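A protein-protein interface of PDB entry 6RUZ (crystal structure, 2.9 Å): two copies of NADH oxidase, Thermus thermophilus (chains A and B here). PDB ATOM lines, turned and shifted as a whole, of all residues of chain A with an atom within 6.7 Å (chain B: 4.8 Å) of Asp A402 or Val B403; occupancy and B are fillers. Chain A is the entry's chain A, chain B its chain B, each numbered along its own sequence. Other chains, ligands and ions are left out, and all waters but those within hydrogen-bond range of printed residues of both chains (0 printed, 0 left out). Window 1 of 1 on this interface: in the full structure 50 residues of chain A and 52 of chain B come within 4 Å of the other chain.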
ATOM      1  N   THR A 326      -7.250  25.584  29.628  1.00  0.00           N
ATOM      2  CA  THR A 326      -6.074  26.423  30.003  1.00  0.00           C
ATOM      3  C   THR A 326      -6.314  27.901  29.786  1.00  0.00           C
ATOM      4  O   THR A 326      -6.715  28.254  28.726  1.00  0.00           O
ATOM      5  CB  THR A 326      -4.886  25.969  29.191  1.00  0.00           C
ATOM      6  OG1 THR A 326      -4.846  24.521  29.235  1.00  0.00           O
ATOM      7  CG2 THR A 326      -3.674  26.524  29.677  1.00  0.00           C
ATOM      8  N   THR A 339      -5.633  25.533  34.593  1.00  0.00           N
ATOM      9  CA  THR A 339      -6.024  24.541  33.629  1.00  0.00           C
ATOM     10  C   THR A 339      -6.765  23.358  34.306  1.00  0.00           C
ATOM     11  O   THR A 339      -6.521  22.981  35.517  1.00  0.00           O
ATOM     12  CB  THR A 339      -4.779  24.065  32.788  1.00  0.00           C
ATOM     13  OG1 THR A 339      -5.236  23.322  31.638  1.00  0.00           O
ATOM     14  CG2 THR A 339      -3.747  23.226  33.634  1.00  0.00           C
ATOM     15  N   VAL A 391      -0.451  27.534  37.804  1.00  0.00           N
ATOM     16  CA  VAL A 391       0.765  28.135  38.276  1.00  0.00           C
ATOM     17  C   VAL A 391       0.648  29.676  38.352  1.00  0.00           C
ATOM     18  O   VAL A 391       0.033  30.316  37.520  1.00  0.00           O
ATOM     19  CB  VAL A 391       2.007  27.565  37.603  1.00  0.00           C
ATOM     20  CG1 VAL A 391       1.658  26.580  36.575  1.00  0.00           C
ATOM     21  CG2 VAL A 391       3.017  28.674  37.227  1.00  0.00           C
ATOM     22  N   ALA A 398       5.880  31.467  32.586  1.00  0.00           N
ATOM     23  CA  ALA A 398       5.466  30.461  33.648  1.00  0.00           C
ATOM     24  C   ALA A 398       3.860  30.566  33.716  1.00  0.00           C
ATOM     25  O   ALA A 398       3.366  31.388  34.481  1.00  0.00           O
ATOM     26  CB  ALA A 398       6.207  30.576  34.853  1.00  0.00           C
ATOM     27  N   LEU A 399       3.131  29.590  33.070  1.00  0.00           N
ATOM     28  CA  LEU A 399       3.338  29.275  31.559  1.00  0.00           C
ATOM     29  C   LEU A 399       4.059  27.874  31.453  1.00  0.00           C
ATOM     30  O   LEU A 399       4.042  27.190  30.390  1.00  0.00           O
ATOM     31  CB  LEU A 399       4.384  30.136  30.726  1.00  0.00           C
ATOM     32  CG  LEU A 399       3.904  30.505  29.306  1.00  0.00           C
ATOM     33  CD1 LEU A 399       2.351  31.130  29.132  1.00  0.00           C
ATOM     34  CD2 LEU A 399       4.882  31.453  28.565  1.00  0.00           C
ATOM     35  N   ARG A 400       4.823  27.529  32.515  1.00  0.00           N
ATOM     36  CA  ARG A 400       4.919  26.167  32.956  1.00  0.00           C
ATOM     37  C   ARG A 400       3.491  25.471  32.824  1.00  0.00           C
ATOM     38  O   ARG A 400       3.420  24.273  32.582  1.00  0.00           O
ATOM     39  CB  ARG A 400       5.461  26.181  34.402  1.00  0.00           C
ATOM     40  CG  ARG A 400       6.851  25.666  34.480  1.00  0.00           C
ATOM     41  CD  ARG A 400       7.617  25.862  35.768  1.00  0.00           C
ATOM     42  NE  ARG A 400       8.165  27.159  35.830  1.00  0.00           N
ATOM     43  CZ  ARG A 400       9.436  27.461  35.962  1.00  0.00           C
ATOM     44  NH1 ARG A 400      10.358  26.573  36.128  1.00  0.00           N
ATOM     45  NH2 ARG A 400       9.750  28.755  35.968  1.00  0.00           N
ATOM     46  N   ILE A 401       2.376  26.226  32.970  1.00  0.00           N
ATOM     47  CA  ILE A 401       1.003  25.671  32.888  1.00  0.00           C
ATOM     48  C   ILE A 401       0.855  24.839  31.645  1.00  0.00           C
ATOM     49  O   ILE A 401       0.077  23.931  31.609  1.00  0.00           O
ATOM     50  CB  ILE A 401      -0.126  26.738  32.887  1.00  0.00           C
ATOM     51  CG1 ILE A 401      -1.439  26.094  33.239  1.00  0.00           C
ATOM     52  CG2 ILE A 401      -0.306  27.310  31.533  1.00  0.00           C
ATOM     53  CD1 ILE A 401      -1.669  25.816  34.711  1.00  0.00           C
ATOM     54  N   ASP A 402       1.624  25.157  30.623  1.00  0.00           N
ATOM     55  CA  ASP A 402       1.491  24.471  29.340  1.00  0.00           C
ATOM     56  C   ASP A 402       1.817  22.976  29.446  1.00  0.00           C
ATOM     57  O   ASP A 402       1.254  22.195  28.732  1.00  0.00           O
ATOM     58  CB  ASP A 402       2.225  25.214  28.157  1.00  0.00           C
ATOM     59  CG  ASP A 402       1.452  26.446  27.670  1.00  0.00           C
ATOM     60  OD1 ASP A 402       0.228  26.579  28.063  1.00  0.00           O
ATOM     61  OD2 ASP A 402       2.016  27.281  26.901  1.00  0.00           O
ATOM     62  N   VAL A 403       2.682  22.602  30.373  1.00  0.00           N
ATOM     63  CA  VAL A 403       3.136  21.271  30.548  1.00  0.00           C
ATOM     64  C   VAL A 403       1.971  20.566  31.122  1.00  0.00           C
ATOM     65  O   VAL A 403       1.649  19.486  30.706  1.00  0.00           O
ATOM     66  CB  VAL A 403       4.341  21.221  31.542  1.00  0.00           C
ATOM     67  CG1 VAL A 403       4.834  19.810  31.843  1.00  0.00           C
ATOM     68  CG2 VAL A 403       5.507  21.965  30.929  1.00  0.00           C
ATOM     69  N   LEU A 404       1.295  21.168  32.065  1.00  0.00           N
ATOM     70  CA  LEU A 404       0.129  20.476  32.620  1.00  0.00           C
ATOM     71  C   LEU A 404      -1.005  20.258  31.585  1.00  0.00           C
ATOM     72  O   LEU A 404      -1.622  19.210  31.535  1.00  0.00           O
ATOM     73  CB  LEU A 404      -0.425  21.186  33.865  1.00  0.00           C
ATOM     74  CG  LEU A 404       0.439  21.416  35.077  1.00  0.00           C
ATOM     75  CD1 LEU A 404      -0.233  22.326  36.091  1.00  0.00           C
ATOM     76  CD2 LEU A 404       0.804  20.033  35.637  1.00  0.00           C
ATOM     77  N   ALA A 405      -1.268  21.280  30.781  1.00  0.00           N
ATOM     78  CA  ALA A 405      -2.255  21.206  29.749  1.00  0.00           C
ATOM     79  C   ALA A 405      -1.869  20.013  28.887  1.00  0.00           C
ATOM     80  O   ALA A 405      -2.741  19.228  28.495  1.00  0.00           O
ATOM     81  CB  ALA A 405      -2.339  22.516  28.933  1.00  0.00           C
ATOM     82  N   ALA A 406      -0.587  19.846  28.636  1.00  0.00           N
ATOM     83  CA  ALA A 406      -0.111  18.739  27.783  1.00  0.00           C
ATOM     84  C   ALA A 406      -0.458  17.324  28.332  1.00  0.00           C
ATOM     85  O   ALA A 406      -0.878  16.417  27.619  1.00  0.00           O
ATOM     86  CB  ALA A 406       1.446  18.869  27.538  1.00  0.00           C
ATOM     87  N   LEU A 407      -0.265  17.181  29.627  1.00  0.00           N
ATOM     88  CA  LEU A 407      -0.462  15.976  30.306  1.00  0.00           C
ATOM     89  C   LEU A 407      -1.935  15.622  30.456  1.00  0.00           C
ATOM     90  O   LEU A 407      -2.329  14.468  30.352  1.00  0.00           O
ATOM     91  CB  LEU A 407       0.139  16.157  31.660  1.00  0.00           C
ATOM     92  CG  LEU A 407       1.621  15.885  31.856  1.00  0.00           C
ATOM     93  CD1 LEU A 407       1.974  16.253  33.275  1.00  0.00           C
ATOM     94  CD2 LEU A 407       1.910  14.442  31.567  1.00  0.00           C
ATOM     95  N   LEU A 422      12.533  18.123  32.662  1.00  0.00           N
ATOM     96  CA  LEU A 422      12.378  19.541  32.383  1.00  0.00           C
ATOM     97  C   LEU A 422      13.729  20.277  32.450  1.00  0.00           C
ATOM     98  O   LEU A 422      14.800  19.682  32.786  1.00  0.00           O
ATOM     99  CB  LEU A 422      11.462  20.126  33.391  1.00  0.00           C
ATOM    100  CG  LEU A 422      10.217  19.325  33.688  1.00  0.00           C
ATOM    101  CD1 LEU A 422       9.471  20.050  34.691  1.00  0.00           C
ATOM    102  CD2 LEU A 422       9.408  19.124  32.453  1.00  0.00           C
ATOM    103  N   ARG B 400       8.977  27.064  27.166  1.00  0.00           N
ATOM    104  CA  ARG B 400       8.005  26.361  26.401  1.00  0.00           C
ATOM    105  C   ARG B 400       8.668  24.970  26.114  1.00  0.00           C
ATOM    106  O   ARG B 400       8.053  23.968  25.669  1.00  0.00           O
ATOM    107  CB  ARG B 400       7.721  27.244  25.156  1.00  0.00           C
ATOM    108  CG  ARG B 400       6.333  27.840  25.159  1.00  0.00           C
ATOM    109  CD  ARG B 400       5.982  28.867  24.044  1.00  0.00           C
ATOM    110  NE  ARG B 400       6.450  30.137  24.523  1.00  0.00           N
ATOM    111  CZ  ARG B 400       5.675  31.199  24.666  1.00  0.00           C
ATOM    112  NH1 ARG B 400       4.374  31.151  24.331  1.00  0.00           N
ATOM    113  NH2 ARG B 400       6.213  32.328  25.118  1.00  0.00           N
ATOM    114  N   ILE B 401       9.975  24.899  26.306  1.00  0.00           N
ATOM    115  CA  ILE B 401      10.666  23.669  25.858  1.00  0.00           C
ATOM    116  C   ILE B 401      10.101  22.502  26.672  1.00  0.00           C
ATOM    117  O   ILE B 401      10.119  21.378  26.320  1.00  0.00           O
ATOM    118  CB  ILE B 401      12.231  23.779  26.023  1.00  0.00           C
ATOM    119  CG1 ILE B 401      12.947  22.637  25.336  1.00  0.00           C
ATOM    120  CG2 ILE B 401      12.591  23.640  27.435  1.00  0.00           C
ATOM    121  CD1 ILE B 401      13.181  22.857  23.885  1.00  0.00           C
ATOM    122  N   ASP B 402       9.606  22.811  27.824  1.00  0.00           N
ATOM    123  CA  ASP B 402       9.166  21.769  28.709  1.00  0.00           C
ATOM    124  C   ASP B 402       7.988  20.979  28.104  1.00  0.00           C
ATOM    125  O   ASP B 402       7.863  19.814  28.357  1.00  0.00           O
ATOM    126  CB  ASP B 402       8.880  22.280  30.186  1.00  0.00           C
ATOM    127  CG  ASP B 402      10.182  22.647  30.941  1.00  0.00           C
ATOM    128  OD1 ASP B 402      11.254  22.212  30.453  1.00  0.00           O
ATOM    129  OD2 ASP B 402      10.172  23.325  32.033  1.00  0.00           O
ATOM    130  N   VAL B 403       7.147  21.613  27.303  1.00  0.00           N
ATOM    131  CA  VAL B 403       6.018  20.991  26.673  1.00  0.00           C
ATOM    132  C   VAL B 403       6.535  19.904  25.733  1.00  0.00           C
ATOM    133  O   VAL B 403       5.890  18.866  25.501  1.00  0.00           O
ATOM    134  CB  VAL B 403       5.234  22.060  25.810  1.00  0.00           C
ATOM    135  CG1 VAL B 403       4.000  21.425  25.176  1.00  0.00           C
ATOM    136  CG2 VAL B 403       4.776  23.147  26.632  1.00  0.00           C
ATOM    137  N   LEU B 404       7.698  20.162  25.138  1.00  0.00           N
ATOM    138  CA  LEU B 404       8.151  19.247  24.094  1.00  0.00           C
ATOM    139  C   LEU B 404       8.730  18.074  24.795  1.00  0.00           C
ATOM    140  O   LEU B 404       8.572  16.932  24.356  1.00  0.00           O
ATOM    141  CB  LEU B 404       9.189  19.881  23.156  1.00  0.00           C
ATOM    142  CG  LEU B 404       8.766  20.993  22.226  1.00  0.00           C
ATOM    143  CD1 LEU B 404      10.063  21.494  21.572  1.00  0.00           C
ATOM    144  CD2 LEU B 404       7.673  20.534  21.306  1.00  0.00           C
ATOM    145  N   ALA B 405       9.465  18.402  25.855  1.00  0.00           N
ATOM    146  CA  ALA B 405      10.095  17.437  26.718  1.00  0.00           C
ATOM    147  C   ALA B 405       8.980  16.514  27.191  1.00  0.00           C
ATOM    148  O   ALA B 405       9.056  15.306  27.144  1.00  0.00           O
ATOM    149  CB  ALA B 405      10.805  18.163  27.862  1.00  0.00           C
ATOM    150  N   ALA B 406       7.902  17.101  27.582  1.00  0.00           N
ATOM    151  CA  ALA B 406       6.726  16.336  27.945  1.00  0.00           C
ATOM    152  C   ALA B 406       6.263  15.389  26.928  1.00  0.00           C
ATOM    153  O   ALA B 406       6.079  14.226  27.259  1.00  0.00           O
ATOM    154  CB  ALA B 406       5.545  17.262  28.337  1.00  0.00           C
ATOM    155  N   LEU B 407       5.967  15.873  25.750  1.00  0.00           N
ATOM    156  CA  LEU B 407       5.571  15.002  24.649  1.00  0.00           C
ATOM    157  C   LEU B 407       6.573  13.928  24.259  1.00  0.00           C
ATOM    158  O   LEU B 407       6.178  12.828  23.943  1.00  0.00           O
ATOM    159  CB  LEU B 407       5.326  15.831  23.399  1.00  0.00           C
ATOM    160  CG  LEU B 407       4.136  16.743  23.303  1.00  0.00           C
ATOM    161  CD1 LEU B 407       4.323  17.525  22.091  1.00  0.00           C
ATOM    162  CD2 LEU B 407       2.926  15.849  23.140  1.00  0.00           C
ATOM    163  N   LEU B 417       1.064  17.649  19.450  1.00  0.00           N
ATOM    164  CA  LEU B 417       1.400  19.011  19.733  1.00  0.00           C
ATOM    165  C   LEU B 417       0.345  19.972  19.189  1.00  0.00           C
ATOM    166  O   LEU B 417      -0.197  20.723  19.900  1.00  0.00           O
ATOM    167  CB  LEU B 417       2.804  19.335  19.228  1.00  0.00           C
ATOM    168  CG  LEU B 417       3.247  20.800  19.348  1.00  0.00           C
ATOM    169  CD1 LEU B 417       3.186  21.185  20.766  1.00  0.00           C
ATOM    170  CD2 LEU B 417       4.637  20.896  18.932  1.00  0.00           C
ATOM    171  N   LEU B 420      -2.930  20.370  21.486  1.00  0.00           N
ATOM    172  CA  LEU B 420      -2.704  20.961  22.786  1.00  0.00           C
ATOM    173  C   LEU B 420      -3.438  22.287  22.933  1.00  0.00           C
ATOM    174  O   LEU B 420      -3.420  23.193  22.069  1.00  0.00           O
ATOM    175  CB  LEU B 420      -1.190  21.179  23.026  1.00  0.00           C
ATOM    176  CG  LEU B 420      -0.464  19.910  23.422  1.00  0.00           C
ATOM    177  CD1 LEU B 420       0.846  20.262  24.131  1.00  0.00           C
ATOM    178  CD2 LEU B 420      -1.378  18.918  24.214  1.00  0.00           C
ATOM    179  N   LEU B 422      -2.905  25.242  24.613  1.00  0.00           N
ATOM    180  CA  LEU B 422      -2.017  26.101  25.470  1.00  0.00           C
ATOM    181  C   LEU B 422      -2.602  27.449  25.873  1.00  0.00           C
ATOM    182  O   LEU B 422      -3.780  27.841  25.530  1.00  0.00           O
ATOM    183  CB  LEU B 422      -0.678  26.385  24.819  1.00  0.00           C
ATOM    184  CG  LEU B 422      -0.167  25.154  24.026  1.00  0.00           C
ATOM    185  CD1 LEU B 422       1.011  25.567  23.205  1.00  0.00           C
ATOM    186  CD2 LEU B 422       0.160  23.962  24.810  1.00  0.00           C
ATOM    187  N   ALA B 423      -1.782  28.197  26.596  1.00  0.00           N
ATOM    188  CA  ALA B 423      -2.333  29.422  27.218  1.00  0.00           C
ATOM    189  C   ALA B 423      -2.030  30.607  26.405  1.00  0.00           C
ATOM    190  O   ALA B 423      -0.876  30.823  26.058  1.00  0.00           O
ATOM    191  CB  ALA B 423      -1.803  29.638  28.580  1.00  0.00           C
ATOM    192  N   ASP B 433       0.213  29.841  19.847  1.00  0.00           N
ATOM    193  CA  ASP B 433       1.472  29.772  20.529  1.00  0.00           C
ATOM    194  C   ASP B 433       2.521  29.447  19.511  1.00  0.00           C
ATOM    195  O   ASP B 433       2.208  28.655  18.598  1.00  0.00           O
ATOM    196  CB  ASP B 433       1.485  28.640  21.523  1.00  0.00           C
ATOM    197  CG  ASP B 433       2.624  28.778  22.512  1.00  0.00           C
ATOM    198  OD1 ASP B 433       3.808  28.404  22.216  1.00  0.00           O
ATOM    199  OD2 ASP B 433       2.304  29.341  23.572  1.00  0.00           O
ATOM    200  N   LEU B 435       4.852  27.263  19.644  1.00  0.00           N
ATOM    201  CA  LEU B 435       4.818  25.818  19.447  1.00  0.00           C
ATOM    202  C   LEU B 435       3.754  25.430  18.436  1.00  0.00           C
ATOM    203  O   LEU B 435       4.007  24.713  17.502  1.00  0.00           O
ATOM    204  CB  LEU B 435       4.507  25.129  20.737  1.00  0.00           C
ATOM    205  CG  LEU B 435       5.684  25.326  21.718  1.00  0.00           C
ATOM    206  CD1 LEU B 435       5.195  25.093  23.161  1.00  0.00           C
ATOM    207  CD2 LEU B 435       6.935  24.529  21.428  1.00  0.00           C
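The backbone NH of Ala B423 lies within hydrogen-bond range of the side-chain carboxylate of Asp A402, 3.0 Å away.
OD1 of Asp B433 is in hydrogen-bond range of N of Leu B435, 3.0 Å away. OG1 of Thr A326 lies within hydrogen-bond range of OG1 of Thr A339 (2.7 Å). NH1 of Arg B400 is in salt-bridge range of OD2 of Asp B433 (2.9 Å).
CB of Ala B423 touches CG2 of Thr A326 (3.8 Å). Leu A399 touches Arg B400 (CD2 to NH2, 3.8 Å). CG2 of Val B403 touches CB of Asp A402, at 3.6 Å. Asp A402 touches Leu B422. OD2 of Asp A402 touches OD2 of Asp B433 (3.9 Å). CB of Asp B402 touches CG2 of Val A403, at 3.5 Å. Val A403 touches Val B403 (CG2 to N, 3.995 Å). CB of Ala A406 touches CD1 of Leu B420, at 3.7 Å. CA of Leu A422 touches OD1 of Asp B402 (3.5 Å).
Of chain B, only Val B403, Leu B422, Ala B423 and Asp B433 come within 4 Å of Asp A402. Printed residues of chain A within 4 Å of Val B403: Asp A402 and Val A403. Printed residues of chain A within 4 Å of Asp B402: Val A403 and Leu A422. Of the printed residues of chain A, Leu B420 touches Ala A406. Of the printed residues of chain B, Val A403 touches Asp B402 (3.5 Å) and Val B403 (3.995 Å). Of the printed residues of chain A, Leu B422 touches Asp A402. Leu B417 touches none of the printed residues of chain A. The nearest residue of chain B that does not touch Asp A402 is Arg B400 (4.7 Å).
Of the 14 printed residues of chain B, 7 touch a printed residue of chain A. Hydrophobic or aromatic side chains of chain A within 4 Å of the printed part of chain B: Leu A399, Val A403, Ala A406 and Leu A422. Along chain A the printed residues that touch a printed residue of chain B span positions 326 to 422. Among the printed residues, 10 pairs touch across the chains.
Asp A402 touches Val B403, and with the chains exchanged Val A403 touches Asp B402. Asp A402 touches Leu B422, and with the chains exchanged Leu A422 touches Asp B402. Val A403 touches its own counterpart, Val B403. Positions printed for both chains: 400, 401, 402, 403, 404, 405, 406, 407 and 422. Of the 10 pairs that touch across the chains among the printed residues, 5 have their exchanged pair printed and touching as well.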
